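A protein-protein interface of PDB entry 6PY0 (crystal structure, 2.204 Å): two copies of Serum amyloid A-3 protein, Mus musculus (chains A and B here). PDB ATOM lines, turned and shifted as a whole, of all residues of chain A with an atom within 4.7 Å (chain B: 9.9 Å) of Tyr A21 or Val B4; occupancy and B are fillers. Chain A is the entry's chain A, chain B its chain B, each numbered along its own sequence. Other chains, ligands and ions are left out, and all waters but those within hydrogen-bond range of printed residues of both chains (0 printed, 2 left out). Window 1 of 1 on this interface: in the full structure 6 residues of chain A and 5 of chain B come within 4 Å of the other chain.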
ATOM      1  N   MET A  17      -3.323 -26.500 -20.708  1.00  0.00           N
ATOM      2  CA  MET A  17      -3.988 -27.313 -19.721  1.00  0.00           C
ATOM      3  C   MET A  17      -5.527 -27.341 -19.952  1.00  0.00           C
ATOM      4  O   MET A  17      -6.105 -28.404 -19.934  1.00  0.00           O
ATOM      5  CB  MET A  17      -3.587 -26.914 -18.302  1.00  0.00           C
ATOM      6  CG  MET A  17      -2.137 -27.198 -17.923  1.00  0.00           C
ATOM      7  SD  MET A  17      -1.543 -28.860 -17.932  1.00  0.00           S
ATOM      8  CE  MET A  17      -2.437 -29.536 -16.578  1.00  0.00           C
ATOM      9  N   TRP A  18      -6.157 -26.199 -20.201  1.00  0.00           N
ATOM     10  CA  TRP A  18      -7.585 -26.196 -20.394  1.00  0.00           C
ATOM     11  C   TRP A  18      -7.933 -26.912 -21.664  1.00  0.00           C
ATOM     12  O   TRP A  18      -8.921 -27.519 -21.739  1.00  0.00           O
ATOM     13  CB  TRP A  18      -8.214 -24.820 -20.335  1.00  0.00           C
ATOM     14  CG  TRP A  18      -7.801 -23.961 -19.192  1.00  0.00           C
ATOM     15  CD1 TRP A  18      -7.501 -22.671 -19.255  1.00  0.00           C
ATOM     16  CD2 TRP A  18      -7.667 -24.327 -17.839  1.00  0.00           C
ATOM     17  NE1 TRP A  18      -7.162 -22.204 -18.057  1.00  0.00           N
ATOM     18  CE2 TRP A  18      -7.254 -23.210 -17.159  1.00  0.00           C
ATOM     19  CE3 TRP A  18      -7.814 -25.511 -17.139  1.00  0.00           C
ATOM     20  CZ2 TRP A  18      -7.017 -23.216 -15.820  1.00  0.00           C
ATOM     21  CZ3 TRP A  18      -7.578 -25.510 -15.827  1.00  0.00           C
ATOM     22  CH2 TRP A  18      -7.192 -24.374 -15.173  1.00  0.00           C
ATOM     23  N   ARG A  19      -7.051 -26.874 -22.625  1.00  0.00           N
ATOM     24  CA  ARG A  19      -7.284 -27.504 -23.916  1.00  0.00           C
ATOM     25  C   ARG A  19      -7.238 -29.027 -23.790  1.00  0.00           C
ATOM     26  O   ARG A  19      -8.032 -29.734 -24.408  1.00  0.00           O
ATOM     27  CB  ARG A  19      -6.267 -27.010 -24.944  1.00  0.00           C
ATOM     28  CG  ARG A  19      -6.560 -27.433 -26.373  1.00  0.00           C
ATOM     29  CD  ARG A  19      -5.825 -26.534 -27.371  1.00  0.00           C
ATOM     30  NE  ARG A  19      -4.434 -26.296 -26.989  1.00  0.00           N
ATOM     31  CZ  ARG A  19      -3.451 -27.169 -27.179  1.00  0.00           C
ATOM     32  NH1 ARG A  19      -3.707 -28.344 -27.739  1.00  0.00           N
ATOM     33  NH2 ARG A  19      -2.215 -26.874 -26.802  1.00  0.00           N
ATOM     34  N   ALA A  20      -6.309 -29.522 -22.979  1.00  0.00           N
ATOM     35  CA  ALA A  20      -6.197 -30.952 -22.720  1.00  0.00           C
ATOM     36  C   ALA A  20      -7.446 -31.489 -22.029  1.00  0.00           C
ATOM     37  O   ALA A  20      -7.996 -32.507 -22.435  1.00  0.00           O
ATOM     38  CB  ALA A  20      -4.972 -31.246 -21.886  1.00  0.00           C
ATOM     39  N   TYR A  21      -7.877 -30.809 -20.973  1.00  0.00           N
ATOM     40  CA  TYR A  21      -9.081 -31.206 -20.251  1.00  0.00           C
ATOM     41  C   TYR A  21     -10.304 -31.155 -21.170  1.00  0.00           C
ATOM     42  O   TYR A  21     -11.166 -32.030 -21.128  1.00  0.00           O
ATOM     43  CB  TYR A  21      -9.297 -30.312 -19.027  1.00  0.00           C
ATOM     44  CG  TYR A  21      -8.229 -30.453 -17.947  1.00  0.00           C
ATOM     45  CD1 TYR A  21      -7.533 -31.647 -17.769  1.00  0.00           C
ATOM     46  CD2 TYR A  21      -7.927 -29.394 -17.103  1.00  0.00           C
ATOM     47  CE1 TYR A  21      -6.561 -31.776 -16.774  1.00  0.00           C
ATOM     48  CE2 TYR A  21      -6.964 -29.507 -16.113  1.00  0.00           C
ATOM     49  CZ  TYR A  21      -6.281 -30.692 -15.952  1.00  0.00           C
ATOM     50  OH  TYR A  21      -5.328 -30.783 -14.961  1.00  0.00           O
ATOM     51  N   SER A  22     -10.361 -30.132 -22.010  1.00  0.00           N
ATOM     52  CA  SER A  22     -11.460 -29.980 -22.950  1.00  0.00           C
ATOM     53  C   SER A  22     -11.434 -31.104 -23.978  1.00  0.00           C
ATOM     54  O   SER A  22     -12.475 -31.669 -24.318  1.00  0.00           O
ATOM     55  CB  SER A  22     -11.367 -28.630 -23.649  1.00  0.00           C
ATOM     56  OG  SER A  22     -12.394 -28.487 -24.609  1.00  0.00           O
ATOM     57  N   ASP A  23     -10.241 -31.424 -24.469  1.00  0.00           N
ATOM     58  CA  ASP A  23     -10.078 -32.489 -25.452  1.00  0.00           C
ATOM     59  C   ASP A  23     -10.480 -33.837 -24.865  1.00  0.00           C
ATOM     60  O   ASP A  23     -11.113 -34.653 -25.534  1.00  0.00           O
ATOM     61  CB  ASP A  23      -8.633 -32.540 -25.951  1.00  0.00           C
ATOM     62  CG  ASP A  23      -8.389 -31.619 -27.129  1.00  0.00           C
ATOM     63  OD1 ASP A  23      -9.373 -31.076 -27.674  1.00  0.00           O
ATOM     64  OD2 ASP A  23      -7.213 -31.436 -27.509  1.00  0.00           O
ATOM     65  N   MET A  24     -10.130 -34.048 -23.612  1.00  0.00           N
ATOM     66  CA  MET A  24     -10.444 -35.246 -22.864  1.00  0.00           C
ATOM     67  C   MET A  24     -11.949 -35.445 -22.761  1.00  0.00           C
ATOM     68  O   MET A  24     -12.458 -36.552 -22.854  1.00  0.00           O
ATOM     69  CB  MET A  24      -9.799 -35.205 -21.478  1.00  0.00           C
ATOM     70  CG  MET A  24     -10.276 -36.261 -20.526  1.00  0.00           C
ATOM     71  SD  MET A  24      -9.336 -36.457 -19.005  1.00  0.00           S
ATOM     72  CE  MET A  24      -9.084 -34.816 -18.486  1.00  0.00           C
ATOM     73  N   LYS A  25     -12.637 -34.345 -22.597  1.00  0.00           N
ATOM     74  CA  LYS A  25     -14.088 -34.355 -22.452  1.00  0.00           C
ATOM     75  C   LYS A  25     -14.766 -34.694 -23.775  1.00  0.00           C
ATOM     76  O   LYS A  25     -15.663 -35.536 -23.825  1.00  0.00           O
ATOM     77  CB  LYS A  25     -14.584 -33.001 -21.939  1.00  0.00           C
ATOM     78  CG  LYS A  25     -15.398 -33.083 -20.659  1.00  0.00           C
ATOM     79  N   HIS A  37      -3.692 -35.733 -19.352  1.00  0.00           N
ATOM     80  CA  HIS A  37      -2.920 -35.179 -18.250  1.00  0.00           C
ATOM     81  C   HIS A  37      -1.479 -34.965 -18.702  1.00  0.00           C
ATOM     82  O   HIS A  37      -0.919 -33.882 -18.520  1.00  0.00           O
ATOM     83  CB  HIS A  37      -2.969 -36.105 -17.036  1.00  0.00           C
ATOM     84  CG  HIS A  37      -4.310 -36.153 -16.369  1.00  0.00           C
ATOM     85  ND1 HIS A  37      -4.808 -37.296 -15.780  1.00  0.00           N
ATOM     86  CD2 HIS A  37      -5.254 -35.198 -16.195  1.00  0.00           C
ATOM     87  CE1 HIS A  37      -6.002 -37.045 -15.275  1.00  0.00           C
ATOM     88  NE2 HIS A  37      -6.296 -35.778 -15.512  1.00  0.00           N
ATOM     89  N   ILE A  58      -1.616 -26.188 -11.616  1.00  0.00           N
ATOM     90  CA  ILE A  58      -2.912 -26.731 -11.982  1.00  0.00           C
ATOM     91  C   ILE A  58      -2.985 -28.223 -11.643  1.00  0.00           C
ATOM     92  O   ILE A  58      -3.980 -28.700 -11.090  1.00  0.00           O
ATOM     93  CB  ILE A  58      -3.203 -26.488 -13.481  1.00  0.00           C
ATOM     94  CG1 ILE A  58      -3.361 -24.989 -13.751  1.00  0.00           C
ATOM     95  CG2 ILE A  58      -4.440 -27.250 -13.922  1.00  0.00           C
ATOM     96  CD1 ILE A  58      -3.384 -24.621 -15.237  1.00  0.00           C
ATOM     97  N   ARG A  62      -5.403 -29.874  -8.751  1.00  0.00           N
ATOM     98  CA  ARG A  62      -6.311 -30.959  -9.093  1.00  0.00           C
ATOM     99  C   ARG A  62      -6.184 -32.101  -8.101  1.00  0.00           C
ATOM    100  O   ARG A  62      -7.182 -32.617  -7.599  1.00  0.00           O
ATOM    101  CB  ARG A  62      -6.032 -31.464 -10.508  1.00  0.00           C
ATOM    102  CG  ARG A  62      -6.973 -32.567 -10.944  1.00  0.00           C
ATOM    103  CD  ARG A  62      -6.782 -32.927 -12.404  1.00  0.00           C
ATOM    104  NE  ARG A  62      -7.565 -34.108 -12.747  1.00  0.00           N
ATOM    105  CZ  ARG A  62      -7.143 -35.351 -12.539  1.00  0.00           C
ATOM    106  NH1 ARG A  62      -7.909 -36.386 -12.865  1.00  0.00           N
ATOM    107  NH2 ARG A  62      -5.947 -35.558 -12.001  1.00  0.00           N
ATOM    108  N   ARG B   2     -17.073 -27.558 -13.485  1.00  0.00           N
ATOM    109  CA  ARG B   2     -16.249 -28.382 -12.609  1.00  0.00           C
ATOM    110  C   ARG B   2     -15.191 -27.544 -11.898  1.00  0.00           C
ATOM    111  O   ARG B   2     -15.306 -26.321 -11.816  1.00  0.00           O
ATOM    112  CB  ARG B   2     -15.584 -29.509 -13.402  1.00  0.00           C
ATOM    113  CG  ARG B   2     -15.150 -30.692 -12.553  1.00  0.00           C
ATOM    114  CD  ARG B   2     -14.498 -31.772 -13.403  1.00  0.00           C
ATOM    115  NE  ARG B   2     -13.083 -31.935 -13.090  1.00  0.00           N
ATOM    116  CZ  ARG B   2     -12.180 -32.411 -13.940  1.00  0.00           C
ATOM    117  NH1 ARG B   2     -12.543 -32.773 -15.163  1.00  0.00           N
ATOM    118  NH2 ARG B   2     -10.911 -32.525 -13.568  1.00  0.00           N
ATOM    119  N   TRP B   3     -14.160 -28.210 -11.391  1.00  0.00           N
ATOM    120  CA  TRP B   3     -13.089 -27.535 -10.694  1.00  0.00           C
ATOM    121  C   TRP B   3     -12.340 -26.708 -11.739  1.00  0.00           C
ATOM    122  O   TRP B   3     -11.667 -25.729 -11.415  1.00  0.00           O
ATOM    123  CB  TRP B   3     -12.196 -28.596 -10.047  1.00  0.00           C
ATOM    124  CG  TRP B   3     -10.744 -28.283  -9.953  1.00  0.00           C
ATOM    125  CD1 TRP B   3     -10.104 -27.687  -8.908  1.00  0.00           C
ATOM    126  CD2 TRP B   3      -9.736 -28.592 -10.919  1.00  0.00           C
ATOM    127  NE1 TRP B   3      -8.762 -27.594  -9.168  1.00  0.00           N
ATOM    128  CE2 TRP B   3      -8.508 -28.143 -10.396  1.00  0.00           C
ATOM    129  CE3 TRP B   3      -9.753 -29.196 -12.179  1.00  0.00           C
ATOM    130  CZ2 TRP B   3      -7.308 -28.267 -11.096  1.00  0.00           C
ATOM    131  CZ3 TRP B   3      -8.560 -29.327 -12.867  1.00  0.00           C
ATOM    132  CH2 TRP B   3      -7.354 -28.864 -12.324  1.00  0.00           C
ATOM    133  N   VAL B   4     -12.499 -27.104 -13.001  1.00  0.00           N
ATOM    134  CA  VAL B   4     -11.913 -26.397 -14.134  1.00  0.00           C
ATOM    135  C   VAL B   4     -12.399 -24.948 -14.217  1.00  0.00           C
ATOM    136  O   VAL B   4     -11.598 -24.028 -14.380  1.00  0.00           O
ATOM    137  CB  VAL B   4     -12.215 -27.125 -15.461  1.00  0.00           C
ATOM    138  CG1 VAL B   4     -11.958 -26.213 -16.652  1.00  0.00           C
ATOM    139  CG2 VAL B   4     -11.395 -28.403 -15.567  1.00  0.00           C
ATOM    140  N   GLN B   5     -13.685 -24.749 -14.063  1.00  0.00           N
ATOM    141  CA  GLN B   5     -14.217 -23.430 -14.135  1.00  0.00           C
ATOM    142  C   GLN B   5     -13.722 -22.546 -12.972  1.00  0.00           C
ATOM    143  O   GLN B   5     -13.462 -21.403 -13.128  1.00  0.00           O
ATOM    144  CB  GLN B   5     -15.716 -23.512 -14.186  1.00  0.00           C
ATOM    145  CG  GLN B   5     -16.426 -22.219 -13.947  1.00  0.00           C
ATOM    146  CD  GLN B   5     -16.124 -21.205 -15.012  1.00  0.00           C
ATOM    147  OE1 GLN B   5     -15.804 -21.545 -16.139  1.00  0.00           O
ATOM    148  NE2 GLN B   5     -16.236 -19.946 -14.662  1.00  0.00           N
ATOM    149  N   PHE B   6     -13.665 -23.097 -11.781  1.00  0.00           N
ATOM    150  CA  PHE B   6     -13.101 -22.410 -10.657  1.00  0.00           C
ATOM    151  C   PHE B   6     -11.659 -22.008 -10.935  1.00  0.00           C
ATOM    152  O   PHE B   6     -11.280 -20.919 -10.680  1.00  0.00           O
ATOM    153  CB  PHE B   6     -13.201 -23.269  -9.426  1.00  0.00           C
ATOM    154  CG  PHE B   6     -12.755 -22.614  -8.169  1.00  0.00           C
ATOM    155  CD1 PHE B   6     -13.647 -21.950  -7.380  1.00  0.00           C
ATOM    156  CD2 PHE B   6     -11.463 -22.725  -7.745  1.00  0.00           C
ATOM    157  CE1 PHE B   6     -13.263 -21.400  -6.204  1.00  0.00           C
ATOM    158  CE2 PHE B   6     -11.063 -22.160  -6.572  1.00  0.00           C
ATOM    159  CZ  PHE B   6     -11.968 -21.491  -5.802  1.00  0.00           C
ATOM    160  N   MET B   7     -10.887 -22.913 -11.492  1.00  0.00           N
ATOM    161  CA  MET B   7      -9.503 -22.656 -11.777  1.00  0.00           C
ATOM    162  C   MET B   7      -9.300 -21.631 -12.864  1.00  0.00           C
ATOM    163  O   MET B   7      -8.378 -20.893 -12.783  1.00  0.00           O
ATOM    164  CB  MET B   7      -8.751 -23.927 -12.127  1.00  0.00           C
ATOM    165  CG  MET B   7      -8.647 -24.912 -10.996  1.00  0.00           C
ATOM    166  SD  MET B   7      -7.719 -24.421  -9.554  1.00  0.00           S
ATOM    167  CE  MET B   7      -6.126 -24.063 -10.173  1.00  0.00           C
ATOM    168  N   LYS B   8     -10.155 -21.610 -13.859  1.00  0.00           N
ATOM    169  CA  LYS B   8     -10.076 -20.615 -14.865  1.00  0.00           C
ATOM    170  C   LYS B   8     -10.351 -19.277 -14.255  1.00  0.00           C
ATOM    171  O   LYS B   8      -9.735 -18.336 -14.616  1.00  0.00           O
ATOM    172  CB  LYS B   8     -11.036 -20.860 -16.002  1.00  0.00           C
ATOM    173  CG  LYS B   8     -10.597 -21.946 -16.929  1.00  0.00           C
ATOM    174  CD  LYS B   8     -11.563 -22.109 -18.064  1.00  0.00           C
ATOM    175  CE  LYS B   8     -11.249 -23.370 -18.827  1.00  0.00           C
ATOM    176  NZ  LYS B   8     -12.314 -23.616 -19.801  1.00  0.00           N
ATOM    177  N   GLU B   9     -11.271 -19.213 -13.327  1.00  0.00           N
ATOM    178  CA  GLU B   9     -11.534 -17.927 -12.693  1.00  0.00           C
ATOM    179  C   GLU B   9     -10.337 -17.490 -11.860  1.00  0.00           C
ATOM    180  O   GLU B   9     -10.001 -16.311 -11.812  1.00  0.00           O
ATOM    181  CB  GLU B   9     -12.787 -18.010 -11.823  1.00  0.00           C
ATOM    182  CG  GLU B   9     -14.068 -18.187 -12.612  1.00  0.00           C
ATOM    183  CD  GLU B   9     -15.239 -18.610 -11.746  1.00  0.00           C
ATOM    184  OE1 GLU B   9     -15.029 -18.889 -10.546  1.00  0.00           O
ATOM    185  OE2 GLU B   9     -16.373 -18.667 -12.268  1.00  0.00           O
ATOM    186  N   ALA B  10      -9.696 -18.457 -11.213  1.00  0.00           N
ATOM    187  CA  ALA B  10      -8.497 -18.196 -10.426  1.00  0.00           C
ATOM    188  C   ALA B  10      -7.381 -17.668 -11.310  1.00  0.00           C
ATOM    189  O   ALA B  10      -6.662 -16.743 -10.929  1.00  0.00           O
ATOM    190  CB  ALA B  10      -8.045 -19.459  -9.710  1.00  0.00           C
ATOM    191  N   GLY B  11      -7.246 -18.256 -12.495  1.00  0.00           N
ATOM    192  CA  GLY B  11      -6.245 -17.821 -13.453  1.00  0.00           C
ATOM    193  C   GLY B  11      -6.486 -16.394 -13.903  1.00  0.00           C
ATOM    194  O   GLY B  11      -5.556 -15.590 -13.990  1.00  0.00           O
ATOM    195  N   GLN B  12      -7.743 -16.078 -14.194  1.00  0.00           N
ATOM    196  CA  GLN B  12      -8.120 -14.714 -14.545  1.00  0.00           C
ATOM    197  C   GLN B  12      -7.848 -13.772 -13.373  1.00  0.00           C
ATOM    198  O   GLN B  12      -7.323 -12.680 -13.553  1.00  0.00           O
ATOM    199  CB  GLN B  12      -9.603 -14.648 -14.918  1.00  0.00           C
ATOM    200  CG  GLN B  12     -10.015 -15.533 -16.082  1.00  0.00           C
ATOM    201  CD  GLN B  12      -9.731 -14.894 -17.426  1.00  0.00           C
ATOM    202  OE1 GLN B  12      -8.681 -14.281 -17.627  1.00  0.00           O
ATOM    203  NE2 GLN B  12     -10.675 -15.022 -18.355  1.00  0.00           N
ATOM    204  N   GLY B  50     -13.605 -18.259  -8.040  1.00  0.00           N
ATOM    205  CA  GLY B  50     -12.223 -18.632  -8.290  1.00  0.00           C
ATOM    206  C   GLY B  50     -11.296 -17.429  -8.255  1.00  0.00           C
ATOM    207  O   GLY B  50     -10.179 -17.508  -7.746  1.00  0.00           O
ATOM    208  N   GLY B  51     -11.765 -16.313  -8.804  1.00  0.00           N
ATOM    209  CA  GLY B  51     -11.001 -15.081  -8.820  1.00  0.00           C
ATOM    210  C   GLY B  51     -10.839 -14.497  -7.429  1.00  0.00           C
ATOM    211  O   GLY B  51      -9.756 -14.036  -7.072  1.00  0.00           O
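Of the 12 printed residues of chain A, 4 touch a printed residue of chain B.
Printed residues of chain A that touch a printed residue of chain B: Trp A18, Tyr A21, Ile A58 and Arg A62.
Hydrophobic or aromatic side chains of chain A within 4 Å of the printed part of chain B: Trp A18, Tyr A21 and Ile A58.
Of the 13 printed residues of chain B, 5 touch a printed residue of chain A.
Printed residues of chain B that touch a printed residue of chain A: Arg B2, Trp B3, Val B4, Met B7 and Lys B8.
Hydrophobic or aromatic side chains of chain B within 4 Å of the printed part of chain A: Trp B3, Val B4 and Met B7.
Among the printed residues, no Asp or Glu carboxylate lies within 4 Å of a Lys or Arg side-chain nitrogen of the other chain.
No position is printed for both chains.
Of the 7 pairs that touch across the chains among the printed residues, none has its exchanged pair printed and touching as well.
NH1 of Arg A62 lies close to NE2 of His A37, 3.2 Å away.
The side-chain sulfur (SD) of Met B7 lies close to the indole nitrogen (NE1) of Trp B3 (3.4 Å).
Among the printed residues, merely in contact across the chains: Trp A18 with Met B7, Trp A18 with Lys B8, Tyr A21 with Trp B3, Tyr A21 with Val B4, Ile A58 with Trp B3, Arg A62 with Arg B2 and Arg A62 with Trp B3.
Printed residues of chain B within 4 Å of Tyr A21: Trp B3 (3.6 Å) and Val B4 (3.9 Å).
Printed residues of chain A within 4 Å of Arg B2: Arg A62.
Of the printed residues of chain A, Trp B3 touches Tyr A21, Ile A58 and Arg A62.
Of chain A, only Tyr A21 comes within 4 Å of Val B4.
Printed residues of chain A within 4 Å of Met B7: Trp A18 (3.5 Å).
Printed residues of chain A within 4 Å of Lys B8: Trp A18.
The nearest residue of chain B that does not touch Tyr A21 is Arg B2 (5.5 Å).
The nearest residue of chain A that does not touch Val B4 is Trp A18 (4.2 Å).
The nearest printed residue of chain A that does not touch Met B7 is Ile A58 (4.6 Å).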
